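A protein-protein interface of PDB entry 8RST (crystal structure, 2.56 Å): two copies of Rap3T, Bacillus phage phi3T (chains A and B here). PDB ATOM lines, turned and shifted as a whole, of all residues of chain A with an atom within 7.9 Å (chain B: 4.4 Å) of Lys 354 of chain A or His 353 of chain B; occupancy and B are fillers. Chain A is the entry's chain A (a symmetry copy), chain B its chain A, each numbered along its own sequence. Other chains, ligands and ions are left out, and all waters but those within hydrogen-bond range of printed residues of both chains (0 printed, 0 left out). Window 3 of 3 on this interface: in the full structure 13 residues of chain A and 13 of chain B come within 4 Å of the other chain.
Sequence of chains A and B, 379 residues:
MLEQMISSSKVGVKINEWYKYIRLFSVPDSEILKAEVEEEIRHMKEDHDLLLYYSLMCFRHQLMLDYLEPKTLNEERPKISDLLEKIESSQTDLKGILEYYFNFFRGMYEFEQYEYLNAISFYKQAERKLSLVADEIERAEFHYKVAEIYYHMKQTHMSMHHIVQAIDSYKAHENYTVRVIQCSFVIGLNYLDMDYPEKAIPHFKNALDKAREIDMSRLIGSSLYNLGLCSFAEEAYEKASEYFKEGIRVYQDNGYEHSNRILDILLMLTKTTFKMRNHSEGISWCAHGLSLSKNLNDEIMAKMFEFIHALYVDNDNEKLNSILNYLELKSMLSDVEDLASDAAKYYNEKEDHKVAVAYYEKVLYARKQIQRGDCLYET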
ATOM      1  N   TYR A 347     -28.947  -7.732  10.492  1.00  0.00           N
ATOM      2  CA  TYR A 347     -28.728  -6.396  11.037  1.00  0.00           C
ATOM      3  C   TYR A 347     -29.154  -5.316  10.051  1.00  0.00           C
ATOM      4  O   TYR A 347     -29.675  -4.270  10.457  1.00  0.00           O
ATOM      5  CB  TYR A 347     -27.260  -6.229  11.432  1.00  0.00           C
ATOM      6  CG  TYR A 347     -26.923  -6.860  12.765  1.00  0.00           C
ATOM      7  CD1 TYR A 347     -27.797  -6.757  13.839  1.00  0.00           C
ATOM      8  CD2 TYR A 347     -25.742  -7.569  12.948  1.00  0.00           C
ATOM      9  CE1 TYR A 347     -27.501  -7.332  15.061  1.00  0.00           C
ATOM     10  CE2 TYR A 347     -25.437  -8.148  14.168  1.00  0.00           C
ATOM     11  CZ  TYR A 347     -26.322  -8.026  15.219  1.00  0.00           C
ATOM     12  OH  TYR A 347     -26.027  -8.599  16.435  1.00  0.00           O
ATOM     13  N   ASN A 348     -28.945  -5.547   8.752  1.00  0.00           N
ATOM     14  CA  ASN A 348     -29.420  -4.594   7.754  1.00  0.00           C
ATOM     15  C   ASN A 348     -30.942  -4.538   7.734  1.00  0.00           C
ATOM     16  O   ASN A 348     -31.526  -3.471   7.512  1.00  0.00           O
ATOM     17  CB  ASN A 348     -28.876  -4.954   6.371  1.00  0.00           C
ATOM     18  CG  ASN A 348     -29.278  -3.952   5.307  1.00  0.00           C
ATOM     19  OD1 ASN A 348     -28.721  -2.857   5.228  1.00  0.00           O
ATOM     20  ND2 ASN A 348     -30.245  -4.325   4.475  1.00  0.00           N
ATOM     21  N   GLU A 351     -32.194  -2.384  10.413  1.00  0.00           N
ATOM     22  CA  GLU A 351     -31.752  -1.007  10.202  1.00  0.00           C
ATOM     23  C   GLU A 351     -30.551  -0.641  11.070  1.00  0.00           C
ATOM     24  O   GLU A 351     -30.305   0.541  11.330  1.00  0.00           O
ATOM     25  CB  GLU A 351     -32.903  -0.017  10.429  1.00  0.00           C
ATOM     26  CG  GLU A 351     -34.162  -0.361   9.643  1.00  0.00           C
ATOM     27  CD  GLU A 351     -34.659   0.792   8.791  1.00  0.00           C
ATOM     28  OE1 GLU A 351     -34.356   1.955   9.128  1.00  0.00           O
ATOM     29  OE2 GLU A 351     -35.351   0.533   7.784  1.00  0.00           O
ATOM     30  N   ASP A 352     -29.793  -1.637  11.523  1.00  0.00           N
ATOM     31  CA  ASP A 352     -28.547  -1.398  12.248  1.00  0.00           C
ATOM     32  C   ASP A 352     -27.383  -1.438  11.259  1.00  0.00           C
ATOM     33  O   ASP A 352     -26.550  -2.344  11.257  1.00  0.00           O
ATOM     34  CB  ASP A 352     -28.381  -2.424  13.366  1.00  0.00           C
ATOM     35  CG  ASP A 352     -27.458  -1.941  14.471  1.00  0.00           C
ATOM     36  OD1 ASP A 352     -26.666  -1.010  14.219  1.00  0.00           O
ATOM     37  OD2 ASP A 352     -27.524  -2.496  15.587  1.00  0.00           O
ATOM     38  N   HIS A 353     -27.346  -0.412  10.406  1.00  0.00           N
ATOM     39  CA  HIS A 353     -26.429  -0.424   9.272  1.00  0.00           C
ATOM     40  C   HIS A 353     -24.979  -0.251   9.702  1.00  0.00           C
ATOM     41  O   HIS A 353     -24.069  -0.654   8.970  1.00  0.00           O
ATOM     42  CB  HIS A 353     -26.823   0.667   8.275  1.00  0.00           C
ATOM     43  CG  HIS A 353     -28.259   0.611   7.857  1.00  0.00           C
ATOM     44  ND1 HIS A 353     -28.766  -0.403   7.071  1.00  0.00           N
ATOM     45  CD2 HIS A 353     -29.298   1.438   8.121  1.00  0.00           C
ATOM     46  CE1 HIS A 353     -30.055  -0.196   6.868  1.00  0.00           C
ATOM     47  NE2 HIS A 353     -30.403   0.913   7.496  1.00  0.00           N
ATOM     48  N   LYS A 354     -24.742   0.342  10.872  1.00  0.00           N
ATOM     49  CA  LYS A 354     -23.378   0.501  11.368  1.00  0.00           C
ATOM     50  C   LYS A 354     -22.701  -0.853  11.544  1.00  0.00           C
ATOM     51  O   LYS A 354     -21.646  -1.117  10.956  1.00  0.00           O
ATOM     52  CB  LYS A 354     -23.394   1.282  12.684  1.00  0.00           C
ATOM     53  CG  LYS A 354     -22.096   1.224  13.478  1.00  0.00           C
ATOM     54  CD  LYS A 354     -20.919   1.772  12.690  1.00  0.00           C
ATOM     55  CE  LYS A 354     -19.912   2.443  13.607  1.00  0.00           C
ATOM     56  NZ  LYS A 354     -20.491   3.658  14.247  1.00  0.00           N
ATOM     57  N   VAL A 355     -23.299  -1.731  12.352  1.00  0.00           N
ATOM     58  CA  VAL A 355     -22.723  -3.055  12.558  1.00  0.00           C
ATOM     59  C   VAL A 355     -22.987  -3.980  11.378  1.00  0.00           C
ATOM     60  O   VAL A 355     -22.275  -4.979  11.213  1.00  0.00           O
ATOM     61  CB  VAL A 355     -23.253  -3.681  13.859  1.00  0.00           C
ATOM     62  CG1 VAL A 355     -22.978  -2.761  15.042  1.00  0.00           C
ATOM     63  CG2 VAL A 355     -24.740  -3.976  13.742  1.00  0.00           C
ATOM     64  N   ALA A 356     -23.990  -3.676  10.549  1.00  0.00           N
ATOM     65  CA  ALA A 356     -24.232  -4.482   9.357  1.00  0.00           C
ATOM     66  C   ALA A 356     -23.102  -4.332   8.348  1.00  0.00           C
ATOM     67  O   ALA A 356     -22.785  -5.287   7.629  1.00  0.00           O
ATOM     68  CB  ALA A 356     -25.567  -4.096   8.721  1.00  0.00           C
ATOM     69  N   VAL A 357     -22.492  -3.146   8.280  1.00  0.00           N
ATOM     70  CA  VAL A 357     -21.331  -2.944   7.417  1.00  0.00           C
ATOM     71  C   VAL A 357     -20.200  -3.876   7.827  1.00  0.00           C
ATOM     72  O   VAL A 357     -19.590  -4.550   6.987  1.00  0.00           O
ATOM     73  CB  VAL A 357     -20.881  -1.472   7.459  1.00  0.00           C
ATOM     74  CG1 VAL A 357     -19.467  -1.334   6.925  1.00  0.00           C
ATOM     75  CG2 VAL A 357     -21.825  -0.595   6.665  1.00  0.00           C
ATOM     76  N   ALA A 358     -19.911  -3.933   9.131  1.00  0.00           N
ATOM     77  CA  ALA A 358     -18.766  -4.695   9.618  1.00  0.00           C
ATOM     78  C   ALA A 358     -18.857  -6.168   9.242  1.00  0.00           C
ATOM     79  O   ALA A 358     -17.830  -6.806   8.987  1.00  0.00           O
ATOM     80  CB  ALA A 358     -18.644  -4.542  11.133  1.00  0.00           C
ATOM     81  N   TYR A 359     -20.067  -6.726   9.195  1.00  0.00           N
ATOM     82  CA  TYR A 359     -20.209  -8.126   8.816  1.00  0.00           C
ATOM     83  C   TYR A 359     -20.220  -8.309   7.306  1.00  0.00           C
ATOM     84  O   TYR A 359     -19.825  -9.371   6.815  1.00  0.00           O
ATOM     85  CB  TYR A 359     -21.470  -8.714   9.443  1.00  0.00           C
ATOM     86  CG  TYR A 359     -21.311  -8.944  10.924  1.00  0.00           C
ATOM     87  CD1 TYR A 359     -20.137  -9.480  11.434  1.00  0.00           C
ATOM     88  CD2 TYR A 359     -22.317  -8.601  11.815  1.00  0.00           C
ATOM     89  CE1 TYR A 359     -19.975  -9.687  12.788  1.00  0.00           C
ATOM     90  CE2 TYR A 359     -22.163  -8.804  13.173  1.00  0.00           C
ATOM     91  CZ  TYR A 359     -20.990  -9.347  13.653  1.00  0.00           C
ATOM     92  OH  TYR A 359     -20.830  -9.552  15.002  1.00  0.00           O
ATOM     93  N   TYR A 360     -20.660  -7.296   6.555  1.00  0.00           N
ATOM     94  CA  TYR A 360     -20.487  -7.333   5.107  1.00  0.00           C
ATOM     95  C   TYR A 360     -19.012  -7.282   4.736  1.00  0.00           C
ATOM     96  O   TYR A 360     -18.586  -7.904   3.756  1.00  0.00           O
ATOM     97  CB  TYR A 360     -21.241  -6.178   4.452  1.00  0.00           C
ATOM     98  CG  TYR A 360     -22.679  -6.495   4.113  1.00  0.00           C
ATOM     99  CD1 TYR A 360     -22.990  -7.480   3.186  1.00  0.00           C
ATOM    100  CD2 TYR A 360     -23.723  -5.797   4.703  1.00  0.00           C
ATOM    101  CE1 TYR A 360     -24.301  -7.771   2.866  1.00  0.00           C
ATOM    102  CE2 TYR A 360     -25.037  -6.080   4.389  1.00  0.00           C
ATOM    103  CZ  TYR A 360     -25.320  -7.068   3.471  1.00  0.00           C
ATOM    104  OH  TYR A 360     -26.627  -7.355   3.153  1.00  0.00           O
ATOM    105  N   GLU A 361     -18.216  -6.534   5.508  1.00  0.00           N
ATOM    106  CA  GLU A 361     -16.773  -6.526   5.301  1.00  0.00           C
ATOM    107  C   GLU A 361     -16.176  -7.904   5.557  1.00  0.00           C
ATOM    108  O   GLU A 361     -15.285  -8.350   4.825  1.00  0.00           O
ATOM    109  CB  GLU A 361     -16.110  -5.487   6.208  1.00  0.00           C
ATOM    110  CG  GLU A 361     -16.641  -4.068   6.060  1.00  0.00           C
ATOM    111  CD  GLU A 361     -16.030  -3.110   7.070  1.00  0.00           C
ATOM    112  OE1 GLU A 361     -14.814  -2.841   6.980  1.00  0.00           O
ATOM    113  OE2 GLU A 361     -16.762  -2.628   7.959  1.00  0.00           O
ATOM    114  N   ASN B 348     -18.641   4.816   4.377  1.00  0.00           N
ATOM    115  CA  ASN B 348     -18.418   4.253   5.705  1.00  0.00           C
ATOM    116  C   ASN B 348     -17.516   5.156   6.536  1.00  0.00           C
ATOM    117  O   ASN B 348     -17.694   5.268   7.755  1.00  0.00           O
ATOM    118  CB  ASN B 348     -17.822   2.849   5.597  1.00  0.00           C
ATOM    119  CG  ASN B 348     -17.639   2.186   6.948  1.00  0.00           C
ATOM    120  OD1 ASN B 348     -18.601   1.718   7.556  1.00  0.00           O
ATOM    121  ND2 ASN B 348     -16.399   2.137   7.421  1.00  0.00           N
ATOM    122  N   GLU B 351     -19.434   7.904   8.005  1.00  0.00           N
ATOM    123  CA  GLU B 351     -20.429   7.383   8.939  1.00  0.00           C
ATOM    124  C   GLU B 351     -21.826   7.320   8.327  1.00  0.00           C
ATOM    125  O   GLU B 351     -22.825   7.303   9.053  1.00  0.00           O
ATOM    126  CB  GLU B 351     -20.446   8.199  10.238  1.00  0.00           C
ATOM    127  CG  GLU B 351     -19.069   8.360  10.871  1.00  0.00           C
ATOM    128  CD  GLU B 351     -19.029   7.914  12.319  1.00  0.00           C
ATOM    129  OE1 GLU B 351     -20.091   7.924  12.975  1.00  0.00           O
ATOM    130  OE2 GLU B 351     -17.935   7.551  12.800  1.00  0.00           O
ATOM    131  N   ASP B 352     -21.916   7.282   7.000  1.00  0.00           N
ATOM    132  CA  ASP B 352     -23.190   7.087   6.311  1.00  0.00           C
ATOM    133  C   ASP B 352     -23.367   5.600   6.008  1.00  0.00           C
ATOM    134  O   ASP B 352     -23.323   5.150   4.864  1.00  0.00           O
ATOM    135  CB  ASP B 352     -23.243   7.937   5.044  1.00  0.00           C
ATOM    136  CG  ASP B 352     -24.663   8.223   4.590  1.00  0.00           C
ATOM    137  OD1 ASP B 352     -25.580   7.485   5.005  1.00  0.00           O
ATOM    138  OD2 ASP B 352     -24.859   9.184   3.816  1.00  0.00           O
ATOM    139  N   HIS B 353     -23.574   4.837   7.085  1.00  0.00           N
ATOM    140  CA  HIS B 353     -23.543   3.382   6.979  1.00  0.00           C
ATOM    141  C   HIS B 353     -24.750   2.834   6.230  1.00  0.00           C
ATOM    142  O   HIS B 353     -24.684   1.727   5.685  1.00  0.00           O
ATOM    143  CB  HIS B 353     -23.453   2.763   8.373  1.00  0.00           C
ATOM    144  CG  HIS B 353     -22.332   3.305   9.203  1.00  0.00           C
ATOM    145  ND1 HIS B 353     -21.006   3.054   8.918  1.00  0.00           N
ATOM    146  CD2 HIS B 353     -22.336   4.092  10.304  1.00  0.00           C
ATOM    147  CE1 HIS B 353     -20.244   3.660   9.810  1.00  0.00           C
ATOM    148  NE2 HIS B 353     -21.026   4.299  10.661  1.00  0.00           N
ATOM    149  N   LYS B 354     -25.854   3.581   6.193  1.00  0.00           N
ATOM    150  CA  LYS B 354     -27.033   3.137   5.457  1.00  0.00           C
ATOM    151  C   LYS B 354     -26.714   2.951   3.978  1.00  0.00           C
ATOM    152  O   LYS B 354     -26.896   1.862   3.421  1.00  0.00           O
ATOM    153  CB  LYS B 354     -28.171   4.142   5.651  1.00  0.00           C
ATOM    154  CG  LYS B 354     -29.333   3.988   4.678  1.00  0.00           C
ATOM    155  CD  LYS B 354     -29.976   2.615   4.769  1.00  0.00           C
ATOM    156  CE  LYS B 354     -31.466   2.690   4.483  1.00  0.00           C
ATOM    157  NZ  LYS B 354     -32.178   3.472   5.533  1.00  0.00           N
ATOM    158  N   VAL B 355     -26.233   4.009   3.323  1.00  0.00           N
ATOM    159  CA  VAL B 355     -25.886   3.906   1.910  1.00  0.00           C
ATOM    160  C   VAL B 355     -24.560   3.189   1.700  1.00  0.00           C
ATOM    161  O   VAL B 355     -24.303   2.689   0.597  1.00  0.00           O
ATOM    162  CB  VAL B 355     -25.852   5.298   1.256  1.00  0.00           C
ATOM    163  CG1 VAL B 355     -27.183   6.012   1.455  1.00  0.00           C
ATOM    164  CG2 VAL B 355     -24.708   6.125   1.823  1.00  0.00           C
ATOM    165  N   ALA B 356     -23.709   3.121   2.728  1.00  0.00           N
ATOM    166  CA  ALA B 356     -22.462   2.372   2.606  1.00  0.00           C
ATOM    167  C   ALA B 356     -22.723   0.878   2.478  1.00  0.00           C
ATOM    168  O   ALA B 356     -21.968   0.176   1.795  1.00  0.00           O
ATOM    169  CB  ALA B 356     -21.559   2.653   3.806  1.00  0.00           C
ATOM    170  N   VAL B 357     -23.778   0.380   3.128  1.00  0.00           N
ATOM    171  CA  VAL B 357     -24.164  -1.021   2.978  1.00  0.00           C
ATOM    172  C   VAL B 357     -24.497  -1.323   1.523  1.00  0.00           C
ATOM    173  O   VAL B 357     -24.029  -2.316   0.952  1.00  0.00           O
ATOM    174  CB  VAL B 357     -25.352  -1.352   3.900  1.00  0.00           C
ATOM    175  CG1 VAL B 357     -26.021  -2.641   3.460  1.00  0.00           C
ATOM    176  CG2 VAL B 357     -24.902  -1.464   5.340  1.00  0.00           C
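Of chain A, only His 353, Lys 354 and Val 357 come within 4 Å of His 353 of chain B.
Of the printed residues of chain B, Val 357 of chain A touches Asn 348, His 353 and Val 357.
Of the printed residues of chain B, Asn 348 of chain A touches Val 357.
The nearest printed residue of chain A that does not touch Val 357 of chain B is Ala 356 of chain A (4.3 Å).
Asn 348 of chain A touches Val 357 of chain B, and with the chains exchanged Val 357 of chain A touches Asn 348 of chain B.
His 353 of chain A touches its own counterpart, His 353 of chain B.
His 353 of chain A touches Lys 354 of chain B, and with the chains exchanged Lys 354 of chain A touches His 353 of chain B.
His 353 of chain A touches Val 357 of chain B, and with the chains exchanged Val 357 of chain A touches His 353 of chain B.
Of the 9 pairs that touch across the chains among the printed residues, 8 have their exchanged pair printed and touching as well.
Val 357 of chain B touches Asn 348 of chain A (CG1 to OD1, 3.2 Å).
His 353 of chain A touches His 353 of chain B (CB to O, 3.5 Å).
His 353 of chain A touches Lys 354 of chain B.
O of His 353 of chain A touches CG2 of Val 357 of chain B, at 3.8 Å.
NE2 of His 353 of chain B touches CD of Lys 354 of chain A (3.2 Å).
Val 357 of chain A touches Asn 348 of chain B (CG1 to OD1, 3.2 Å).
Val 357 of chain A touches His 353 of chain B.
Val 357 of chain A touches Val 357 of chain B.
Tyr 360 of chain A touches Val 357 of chain B.
A ring nitrogen (ND1) of His 353 of chain A sits at hydrogen-bond distance from the side-chain amide oxygen (OD1) of Asn 348 of chain A.
The side-chain amide oxygen of Asn 348 of chain B sits at hydrogen-bond distance from a ring nitrogen (ND1) of His 353 of chain B.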
